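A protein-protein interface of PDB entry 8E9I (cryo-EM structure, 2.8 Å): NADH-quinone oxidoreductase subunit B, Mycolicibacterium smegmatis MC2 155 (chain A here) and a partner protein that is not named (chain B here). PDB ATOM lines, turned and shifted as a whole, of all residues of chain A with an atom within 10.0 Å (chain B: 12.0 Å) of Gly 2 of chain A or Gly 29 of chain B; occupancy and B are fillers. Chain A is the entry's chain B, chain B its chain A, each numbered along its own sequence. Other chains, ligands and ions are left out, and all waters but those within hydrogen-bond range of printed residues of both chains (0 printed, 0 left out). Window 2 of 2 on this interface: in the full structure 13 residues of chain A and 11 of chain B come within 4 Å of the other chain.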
ATOM      1  N   GLY A   2     -24.731   6.495  17.680  1.00  0.00           N
ATOM      2  CA  GLY A   2     -24.626   6.402  16.238  1.00  0.00           C
ATOM      3  C   GLY A   2     -24.885   7.735  15.574  1.00  0.00           C
ATOM      4  O   GLY A   2     -25.554   8.594  16.143  1.00  0.00           O
ATOM      5  N   LEU A   3     -24.360   7.910  14.363  1.00  0.00           N
ATOM      6  CA  LEU A   3     -24.496   9.196  13.692  1.00  0.00           C
ATOM      7  C   LEU A   3     -25.956   9.571  13.499  1.00  0.00           C
ATOM      8  O   LEU A   3     -26.301  10.757  13.536  1.00  0.00           O
ATOM      9  CB  LEU A   3     -23.781   9.165  12.346  1.00  0.00           C
ATOM     10  CG  LEU A   3     -22.269   8.957  12.405  1.00  0.00           C
ATOM     11  CD1 LEU A   3     -21.677   9.071  11.011  1.00  0.00           C
ATOM     12  CD2 LEU A   3     -21.609   9.940  13.350  1.00  0.00           C
ATOM     13  N   GLU A   4     -26.828   8.583  13.314  1.00  0.00           N
ATOM     14  CA  GLU A   4     -28.234   8.882  13.085  1.00  0.00           C
ATOM     15  C   GLU A   4     -28.829   9.710  14.212  1.00  0.00           C
ATOM     16  O   GLU A   4     -29.817  10.416  13.988  1.00  0.00           O
ATOM     17  CB  GLU A   4     -29.029   7.589  12.919  1.00  0.00           C
ATOM     18  N   GLU A   5     -28.256   9.638  15.414  1.00  0.00           N
ATOM     19  CA  GLU A   5     -28.748  10.430  16.531  1.00  0.00           C
ATOM     20  C   GLU A   5     -28.063  11.785  16.655  1.00  0.00           C
ATOM     21  O   GLU A   5     -28.534  12.624  17.430  1.00  0.00           O
ATOM     22  CB  GLU A   5     -28.574   9.653  17.838  1.00  0.00           C
ATOM     23  N   ARG A   6     -26.986  12.034  15.916  1.00  0.00           N
ATOM     24  CA  ARG A   6     -26.291  13.312  15.995  1.00  0.00           C
ATOM     25  C   ARG A   6     -26.830  14.337  15.011  1.00  0.00           C
ATOM     26  O   ARG A   6     -26.208  15.387  14.826  1.00  0.00           O
ATOM     27  CB  ARG A   6     -24.787  13.122  15.769  1.00  0.00           C
ATOM     28  CG  ARG A   6     -23.958  13.346  17.028  1.00  0.00           C
ATOM     29  CD  ARG A   6     -22.476  13.105  16.800  1.00  0.00           C
ATOM     30  NE  ARG A   6     -22.171  11.706  16.534  1.00  0.00           N
ATOM     31  CZ  ARG A   6     -21.976  10.788  17.470  1.00  0.00           C
ATOM     32  NH1 ARG A   6     -22.066  11.080  18.757  1.00  0.00           N
ATOM     33  NH2 ARG A   6     -21.687   9.542  17.106  1.00  0.00           N
ATOM     34  N   LEU A   7     -27.966  14.065  14.378  1.00  0.00           N
ATOM     35  CA  LEU A   7     -28.535  15.014  13.441  1.00  0.00           C
ATOM     36  C   LEU A   7     -29.066  16.237  14.188  1.00  0.00           C
ATOM     37  O   LEU A   7     -29.408  16.154  15.372  1.00  0.00           O
ATOM     38  CB  LEU A   7     -29.660  14.360  12.647  1.00  0.00           C
ATOM     39  CG  LEU A   7     -29.258  13.746  11.307  1.00  0.00           C
ATOM     40  CD1 LEU A   7     -27.994  12.901  11.442  1.00  0.00           C
ATOM     41  CD2 LEU A   7     -30.399  12.909  10.772  1.00  0.00           C
ATOM     42  N   PRO A   8     -29.145  17.389  13.522  1.00  0.00           N
ATOM     43  CA  PRO A   8     -29.706  18.574  14.179  1.00  0.00           C
ATOM     44  C   PRO A   8     -31.178  18.380  14.508  1.00  0.00           C
ATOM     45  O   PRO A   8     -31.910  17.694  13.792  1.00  0.00           O
ATOM     46  CB  PRO A   8     -29.497  19.686  13.146  1.00  0.00           C
ATOM     47  CG  PRO A   8     -29.410  18.984  11.847  1.00  0.00           C
ATOM     48  CD  PRO A   8     -28.774  17.656  12.123  1.00  0.00           C
ATOM     49  N   LEU A  13     -33.970  15.210  12.022  1.00  0.00           N
ATOM     50  CA  LEU A  13     -33.988  14.297  13.155  1.00  0.00           C
ATOM     51  C   LEU A  13     -35.392  13.778  13.420  1.00  0.00           C
ATOM     52  O   LEU A  13     -35.572  12.606  13.752  1.00  0.00           O
ATOM     53  CB  LEU A  13     -33.431  14.993  14.394  1.00  0.00           C
ATOM     54  CG  LEU A  13     -33.333  14.120  15.642  1.00  0.00           C
ATOM     55  CD1 LEU A  13     -32.511  12.871  15.369  1.00  0.00           C
ATOM     56  CD2 LEU A  13     -32.737  14.911  16.791  1.00  0.00           C
ATOM     57  N   VAL A  16     -36.200  11.151  10.790  1.00  0.00           N
ATOM     58  CA  VAL A  16     -35.403   9.960  11.053  1.00  0.00           C
ATOM     59  C   VAL A  16     -35.970   9.201  12.242  1.00  0.00           C
ATOM     60  O   VAL A  16     -36.041   7.970  12.234  1.00  0.00           O
ATOM     61  CB  VAL A  16     -33.931  10.339  11.276  1.00  0.00           C
ATOM     62  CG1 VAL A  16     -33.167   9.162  11.864  1.00  0.00           C
ATOM     63  CG2 VAL A  16     -33.306  10.794   9.972  1.00  0.00           C
ATOM     64  N   ALA A  20     -37.322   5.438  11.869  1.00  0.00           N
ATOM     65  CA  ALA A  20     -36.658   4.422  12.675  1.00  0.00           C
ATOM     66  C   ALA A  20     -37.632   3.761  13.633  1.00  0.00           C
ATOM     67  O   ALA A  20     -37.591   2.542  13.823  1.00  0.00           O
ATOM     68  CB  ALA A  20     -35.494   5.041  13.441  1.00  0.00           C
ATOM     69  N   ARG A  24     -38.449  -0.181  13.579  1.00  0.00           N
ATOM     70  CA  ARG A  24     -38.168  -0.980  14.761  1.00  0.00           C
ATOM     71  C   ARG A  24     -39.441  -1.572  15.347  1.00  0.00           C
ATOM     72  O   ARG A  24     -39.399  -2.627  15.987  1.00  0.00           O
ATOM     73  CB  ARG A  24     -37.442  -0.131  15.798  1.00  0.00           C
ATOM     74  CG  ARG A  24     -35.997   0.130  15.460  1.00  0.00           C
ATOM     75  CD  ARG A  24     -35.441   1.269  16.275  1.00  0.00           C
ATOM     76  NE  ARG A  24     -33.999   1.391  16.120  1.00  0.00           N
ATOM     77  CZ  ARG A  24     -33.276   2.390  16.604  1.00  0.00           C
ATOM     78  NH1 ARG A  24     -33.828   3.372  17.297  1.00  0.00           N
ATOM     79  NH2 ARG A  24     -31.963   2.398  16.398  1.00  0.00           N
ATOM     80  N   VAL A  92     -28.071  -6.622  21.503  1.00  0.00           N
ATOM     81  CA  VAL A  92     -27.478  -5.355  21.102  1.00  0.00           C
ATOM     82  C   VAL A  92     -28.570  -4.300  21.026  1.00  0.00           C
ATOM     83  O   VAL A  92     -29.670  -4.547  20.524  1.00  0.00           O
ATOM     84  CB  VAL A  92     -26.728  -5.500  19.762  1.00  0.00           C
ATOM     85  CG1 VAL A  92     -25.704  -6.610  19.856  1.00  0.00           C
ATOM     86  CG2 VAL A  92     -27.692  -5.770  18.632  1.00  0.00           C
ATOM     87  N   GLU A  93     -28.265  -3.112  21.530  1.00  0.00           N
ATOM     88  CA  GLU A  93     -29.255  -2.059  21.584  1.00  0.00           C
ATOM     89  C   GLU A  93     -29.660  -1.643  20.175  1.00  0.00           C
ATOM     90  O   GLU A  93     -28.921  -1.864  19.217  1.00  0.00           O
ATOM     91  CB  GLU A  93     -28.707  -0.857  22.347  1.00  0.00           C
ATOM     92  N   PRO A  94     -30.854  -1.060  20.016  1.00  0.00           N
ATOM     93  CA  PRO A  94     -31.852  -0.854  21.063  1.00  0.00           C
ATOM     94  C   PRO A  94     -32.596  -2.140  21.362  1.00  0.00           C
ATOM     95  O   PRO A  94     -32.802  -2.941  20.456  1.00  0.00           O
ATOM     96  CB  PRO A  94     -32.776   0.183  20.451  1.00  0.00           C
ATOM     97  CG  PRO A  94     -32.740  -0.131  19.017  1.00  0.00           C
ATOM     98  CD  PRO A  94     -31.333  -0.552  18.721  1.00  0.00           C
ATOM     99  N   MET A 153     -40.619   7.221  19.933  1.00  0.00           N
ATOM    100  CA  MET A 153     -39.345   7.127  20.626  1.00  0.00           C
ATOM    101  C   MET A 153     -38.426   8.252  20.180  1.00  0.00           C
ATOM    102  O   MET A 153     -38.219   8.424  18.972  1.00  0.00           O
ATOM    103  CB  MET A 153     -38.678   5.780  20.356  1.00  0.00           C
ATOM    104  CG  MET A 153     -37.333   5.630  21.042  1.00  0.00           C
ATOM    105  SD  MET A 153     -36.817   3.919  21.243  1.00  0.00           S
ATOM    106  CE  MET A 153     -36.001   3.634  19.680  1.00  0.00           C
ATOM    107  N   LEU A 155     -34.763  10.439  19.757  1.00  0.00           N
ATOM    108  CA  LEU A 155     -33.385  10.124  19.411  1.00  0.00           C
ATOM    109  C   LEU A 155     -32.511  11.354  19.601  1.00  0.00           C
ATOM    110  O   LEU A 155     -32.966  12.494  19.481  1.00  0.00           O
ATOM    111  CB  LEU A 155     -33.254   9.629  17.964  1.00  0.00           C
ATOM    112  CG  LEU A 155     -33.863   8.268  17.628  1.00  0.00           C
ATOM    113  CD1 LEU A 155     -33.854   8.045  16.133  1.00  0.00           C
ATOM    114  CD2 LEU A 155     -33.113   7.163  18.329  1.00  0.00           C
ATOM    115  N   GLY A 156     -31.241  11.100  19.897  1.00  0.00           N
ATOM    116  CA  GLY A 156     -30.277  12.178  20.011  1.00  0.00           C
ATOM    117  C   GLY A 156     -30.669  13.194  21.064  1.00  0.00           C
ATOM    118  O   GLY A 156     -31.072  12.856  22.184  1.00  0.00           O
ATOM    119  N   VAL A 157     -30.543  14.470  20.696  1.00  0.00           N
ATOM    120  CA  VAL A 157     -30.852  15.547  21.629  1.00  0.00           C
ATOM    121  C   VAL A 157     -32.273  15.396  22.143  1.00  0.00           C
ATOM    122  O   VAL A 157     -32.564  15.683  23.311  1.00  0.00           O
ATOM    123  CB  VAL A 157     -30.634  16.913  20.954  1.00  0.00           C
ATOM    124  CG1 VAL A 157     -31.550  17.067  19.748  1.00  0.00           C
ATOM    125  CG2 VAL A 157     -30.864  18.035  21.951  1.00  0.00           C
ATOM    126  N   VAL B  20     -19.265  -0.486   2.867  1.00  0.00           N
ATOM    127  CA  VAL B  20     -20.097   0.560   3.447  1.00  0.00           C
ATOM    128  C   VAL B  20     -21.171  -0.048   4.333  1.00  0.00           C
ATOM    129  O   VAL B  20     -21.610   0.567   5.306  1.00  0.00           O
ATOM    130  CB  VAL B  20     -20.698   1.440   2.336  1.00  0.00           C
ATOM    131  CG1 VAL B  20     -21.844   2.271   2.871  1.00  0.00           C
ATOM    132  CG2 VAL B  20     -19.627   2.341   1.752  1.00  0.00           C
ATOM    133  N   SER B  21     -21.611  -1.265   4.022  1.00  0.00           N
ATOM    134  CA  SER B  21     -22.578  -1.930   4.885  1.00  0.00           C
ATOM    135  C   SER B  21     -21.982  -2.219   6.252  1.00  0.00           C
ATOM    136  O   SER B  21     -22.620  -1.972   7.279  1.00  0.00           O
ATOM    137  CB  SER B  21     -23.059  -3.221   4.226  1.00  0.00           C
ATOM    138  N   VAL B  22     -20.756  -2.736   6.287  1.00  0.00           N
ATOM    139  CA  VAL B  22     -20.103  -2.983   7.566  1.00  0.00           C
ATOM    140  C   VAL B  22     -19.847  -1.665   8.284  1.00  0.00           C
ATOM    141  O   VAL B  22     -20.003  -1.562   9.508  1.00  0.00           O
ATOM    142  CB  VAL B  22     -18.802  -3.779   7.363  1.00  0.00           C
ATOM    143  CG1 VAL B  22     -18.095  -3.977   8.689  1.00  0.00           C
ATOM    144  CG2 VAL B  22     -19.093  -5.116   6.708  1.00  0.00           C
ATOM    145  N   GLY B  23     -19.446  -0.636   7.537  1.00  0.00           N
ATOM    146  CA  GLY B  23     -19.239   0.665   8.148  1.00  0.00           C
ATOM    147  C   GLY B  23     -20.503   1.211   8.776  1.00  0.00           C
ATOM    148  O   GLY B  23     -20.469   1.800   9.854  1.00  0.00           O
ATOM    149  N   ILE B  24     -21.636   1.036   8.099  1.00  0.00           N
ATOM    150  CA  ILE B  24     -22.913   1.463   8.658  1.00  0.00           C
ATOM    151  C   ILE B  24     -23.239   0.649   9.898  1.00  0.00           C
ATOM    152  O   ILE B  24     -23.675   1.190  10.920  1.00  0.00           O
ATOM    153  CB  ILE B  24     -24.023   1.341   7.600  1.00  0.00           C
ATOM    154  CG1 ILE B  24     -23.883   2.434   6.550  1.00  0.00           C
ATOM    155  CG2 ILE B  24     -25.389   1.408   8.254  1.00  0.00           C
ATOM    156  CD1 ILE B  24     -24.597   2.119   5.273  1.00  0.00           C
ATOM    157  N   ALA B  25     -23.039  -0.665   9.824  1.00  0.00           N
ATOM    158  CA  ALA B  25     -23.254  -1.508  10.991  1.00  0.00           C
ATOM    159  C   ALA B  25     -22.514  -0.954  12.191  1.00  0.00           C
ATOM    160  O   ALA B  25     -23.085  -0.821  13.279  1.00  0.00           O
ATOM    161  CB  ALA B  25     -22.780  -2.930  10.705  1.00  0.00           C
ATOM    162  N   LEU B  26     -21.242  -0.615  12.008  1.00  0.00           N
ATOM    163  CA  LEU B  26     -20.442  -0.149  13.131  1.00  0.00           C
ATOM    164  C   LEU B  26     -20.791   1.281  13.519  1.00  0.00           C
ATOM    165  O   LEU B  26     -20.627   1.667  14.678  1.00  0.00           O
ATOM    166  CB  LEU B  26     -18.959  -0.262  12.794  1.00  0.00           C
ATOM    167  CG  LEU B  26     -18.471  -1.691  12.566  1.00  0.00           C
ATOM    168  CD1 LEU B  26     -17.031  -1.680  12.089  1.00  0.00           C
ATOM    169  CD2 LEU B  26     -18.619  -2.529  13.821  1.00  0.00           C
ATOM    170  N   VAL B  27     -21.278   2.078  12.568  1.00  0.00           N
ATOM    171  CA  VAL B  27     -21.443   3.508  12.796  1.00  0.00           C
ATOM    172  C   VAL B  27     -22.873   3.909  13.139  1.00  0.00           C
ATOM    173  O   VAL B  27     -23.071   4.743  14.033  1.00  0.00           O
ATOM    174  CB  VAL B  27     -20.965   4.291  11.560  1.00  0.00           C
ATOM    175  CG1 VAL B  27     -21.303   5.761  11.691  1.00  0.00           C
ATOM    176  CG2 VAL B  27     -19.474   4.117  11.380  1.00  0.00           C
ATOM    177  N   ILE B  28     -23.869   3.348  12.466  1.00  0.00           N
ATOM    178  CA  ILE B  28     -25.261   3.713  12.689  1.00  0.00           C
ATOM    179  C   ILE B  28     -25.833   2.855  13.804  1.00  0.00           C
ATOM    180  O   ILE B  28     -25.457   1.691  13.984  1.00  0.00           O
ATOM    181  CB  ILE B  28     -26.107   3.572  11.410  1.00  0.00           C
ATOM    182  CG1 ILE B  28     -25.540   4.442  10.287  1.00  0.00           C
ATOM    183  CG2 ILE B  28     -27.542   3.943  11.691  1.00  0.00           C
ATOM    184  CD1 ILE B  28     -25.490   5.922  10.611  1.00  0.00           C
ATOM    185  N   GLY B  29     -26.759   3.442  14.553  1.00  0.00           N
ATOM    186  CA  GLY B  29     -27.395   2.765  15.653  1.00  0.00           C
ATOM    187  C   GLY B  29     -26.686   3.025  16.961  1.00  0.00           C
ATOM    188  O   GLY B  29     -25.570   3.550  16.999  1.00  0.00           O
ATOM    189  N   PRO B  30     -27.318   2.649  18.068  1.00  0.00           N
ATOM    190  CA  PRO B  30     -26.709   2.889  19.377  1.00  0.00           C
ATOM    191  C   PRO B  30     -25.398   2.139  19.524  1.00  0.00           C
ATOM    192  O   PRO B  30     -25.142   1.134  18.859  1.00  0.00           O
ATOM    193  CB  PRO B  30     -27.759   2.364  20.362  1.00  0.00           C
ATOM    194  CG  PRO B  30     -29.026   2.324  19.592  1.00  0.00           C
ATOM    195  CD  PRO B  30     -28.633   2.002  18.192  1.00  0.00           C
ATOM    196  N   ARG B  31     -24.546   2.663  20.390  1.00  0.00           N
ATOM    197  CA  ARG B  31     -23.339   1.975  20.811  1.00  0.00           C
ATOM    198  C   ARG B  31     -23.085   2.282  22.274  1.00  0.00           C
ATOM    199  O   ARG B  31     -22.957   3.447  22.659  1.00  0.00           O
ATOM    200  CB  ARG B  31     -22.131   2.387  19.977  1.00  0.00           C
ATOM    201  CG  ARG B  31     -22.237   2.008  18.521  1.00  0.00           C
ATOM    202  CD  ARG B  31     -20.862   1.837  17.922  1.00  0.00           C
ATOM    203  NE  ARG B  31     -20.325   0.510  18.195  1.00  0.00           N
ATOM    204  CZ  ARG B  31     -19.327   0.256  19.034  1.00  0.00           C
ATOM    205  NH1 ARG B  31     -18.706   1.223  19.692  1.00  0.00           N
ATOM    206  NH2 ARG B  31     -18.944  -1.003  19.220  1.00  0.00           N
ATOM    207  N   ARG B  32     -23.011   1.232  23.085  1.00  0.00           N
ATOM    208  CA  ARG B  32     -22.727   1.391  24.507  1.00  0.00           C
ATOM    209  C   ARG B  32     -21.846   0.233  24.946  1.00  0.00           C
ATOM    210  O   ARG B  32     -22.211  -0.932  24.766  1.00  0.00           O
ATOM    211  CB  ARG B  32     -24.008   1.441  25.328  1.00  0.00           C
ATOM    212  CG  ARG B  32     -23.734   1.607  26.802  1.00  0.00           C
ATOM    213  CD  ARG B  32     -24.972   1.928  27.593  1.00  0.00           C
ATOM    214  NE  ARG B  32     -24.636   2.139  28.995  1.00  0.00           N
ATOM    215  CZ  ARG B  32     -24.009   3.213  29.454  1.00  0.00           C
ATOM    216  NH1 ARG B  32     -23.666   4.209  28.653  1.00  0.00           N
ATOM    217  NH2 ARG B  32     -23.714   3.286  30.747  1.00  0.00           N
ATOM    218  N   PHE B  33     -20.694   0.553  25.524  1.00  0.00           N
ATOM    219  CA  PHE B  33     -19.803  -0.486  26.008  1.00  0.00           C
ATOM    220  C   PHE B  33     -20.429  -1.221  27.183  1.00  0.00           C
ATOM    221  O   PHE B  33     -21.017  -0.614  28.080  1.00  0.00           O
ATOM    222  CB  PHE B  33     -18.463   0.116  26.420  1.00  0.00           C
ATOM    223  CG  PHE B  33     -17.583  -0.836  27.163  1.00  0.00           C
ATOM    224  CD1 PHE B  33     -16.781  -1.730  26.485  1.00  0.00           C
ATOM    225  CD2 PHE B  33     -17.564  -0.841  28.542  1.00  0.00           C
ATOM    226  CE1 PHE B  33     -15.976  -2.612  27.170  1.00  0.00           C
ATOM    227  CE2 PHE B  33     -16.761  -1.715  29.228  1.00  0.00           C
ATOM    228  CZ  PHE B  33     -15.967  -2.604  28.543  1.00  0.00           C
ATOM    229  N   LYS B  37     -22.143  -7.539  27.468  1.00  0.00           N
ATOM    230  CA  LYS B  37     -22.567  -7.557  26.074  1.00  0.00           C
ATOM    231  C   LYS B  37     -21.459  -8.067  25.171  1.00  0.00           C
ATOM    232  O   LYS B  37     -21.713  -8.810  24.218  1.00  0.00           O
ATOM    233  CB  LYS B  37     -22.995  -6.161  25.638  1.00  0.00           C
ATOM    234  CG  LYS B  37     -23.555  -6.108  24.237  1.00  0.00           C
ATOM    235  CD  LYS B  37     -23.710  -4.681  23.749  1.00  0.00           C
ATOM    236  CE  LYS B  37     -24.762  -3.935  24.542  1.00  0.00           C
ATOM    237  NZ  LYS B  37     -24.865  -2.519  24.117  1.00  0.00           N
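The backbone NH of Gly 2 of chain A sits close to the backbone carbonyl oxygen of Gly 29 of chain B, 3.1 Å away. N of Leu 3 of chain A is in hydrogen-bond range of O of Val 27 of chain B (3.4 Å).
Among the printed residues, merely in contact across the chains: Gly 2 of chain A with Val 27 of chain B (3.2 Å), Arg 24 of chain A with Pro 30 of chain B (3.8 Å), Glu 93 of chain A with Pro 30 of chain B (3.9 Å) and Pro 94 of chain A with Pro 30 of chain B (3.8 Å).
Of chain A, only Gly 2 comes within 4 Å of Gly 29 of chain B. Of chain B, only Val 27 comes within 4 Å of Leu 3 of chain A. No residue of chain B comes within 4 Å of Glu 5 of chain A. Glu 93 of chain A touches one residue of chain B. No residue of chain A comes within 4 Å of Ile 28 of chain B. Printed residues of chain A within 4 Å of Pro 30 of chain B: Arg 24 (3.8 Å), Glu 93 (3.9 Å) and Pro 94 (3.8 Å). Of the printed residues of chain A, Val 27 of chain B touches Gly 2 and Leu 3. Of the printed residues of chain B, Pro 94 of chain A touches Pro 30 (3.8 Å). Of the printed residues of chain B, Arg 24 of chain A touches Pro 30 (3.8 Å). The nearest printed residue of chain B that does not touch Gly 2 of chain A is Pro 30 of chain B (4.4 Å). The nearest printed residue of chain A that does not touch Val 27 of chain B is Glu 4 of chain A (5.4 Å).
Printed residues of chain B that touch a printed residue of chain A: Val 27, Gly 29 and Pro 30. Among the printed residues, no Asp or Glu carboxylate lies within 4 Å of a Lys or Arg side-chain nitrogen of the other chain.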
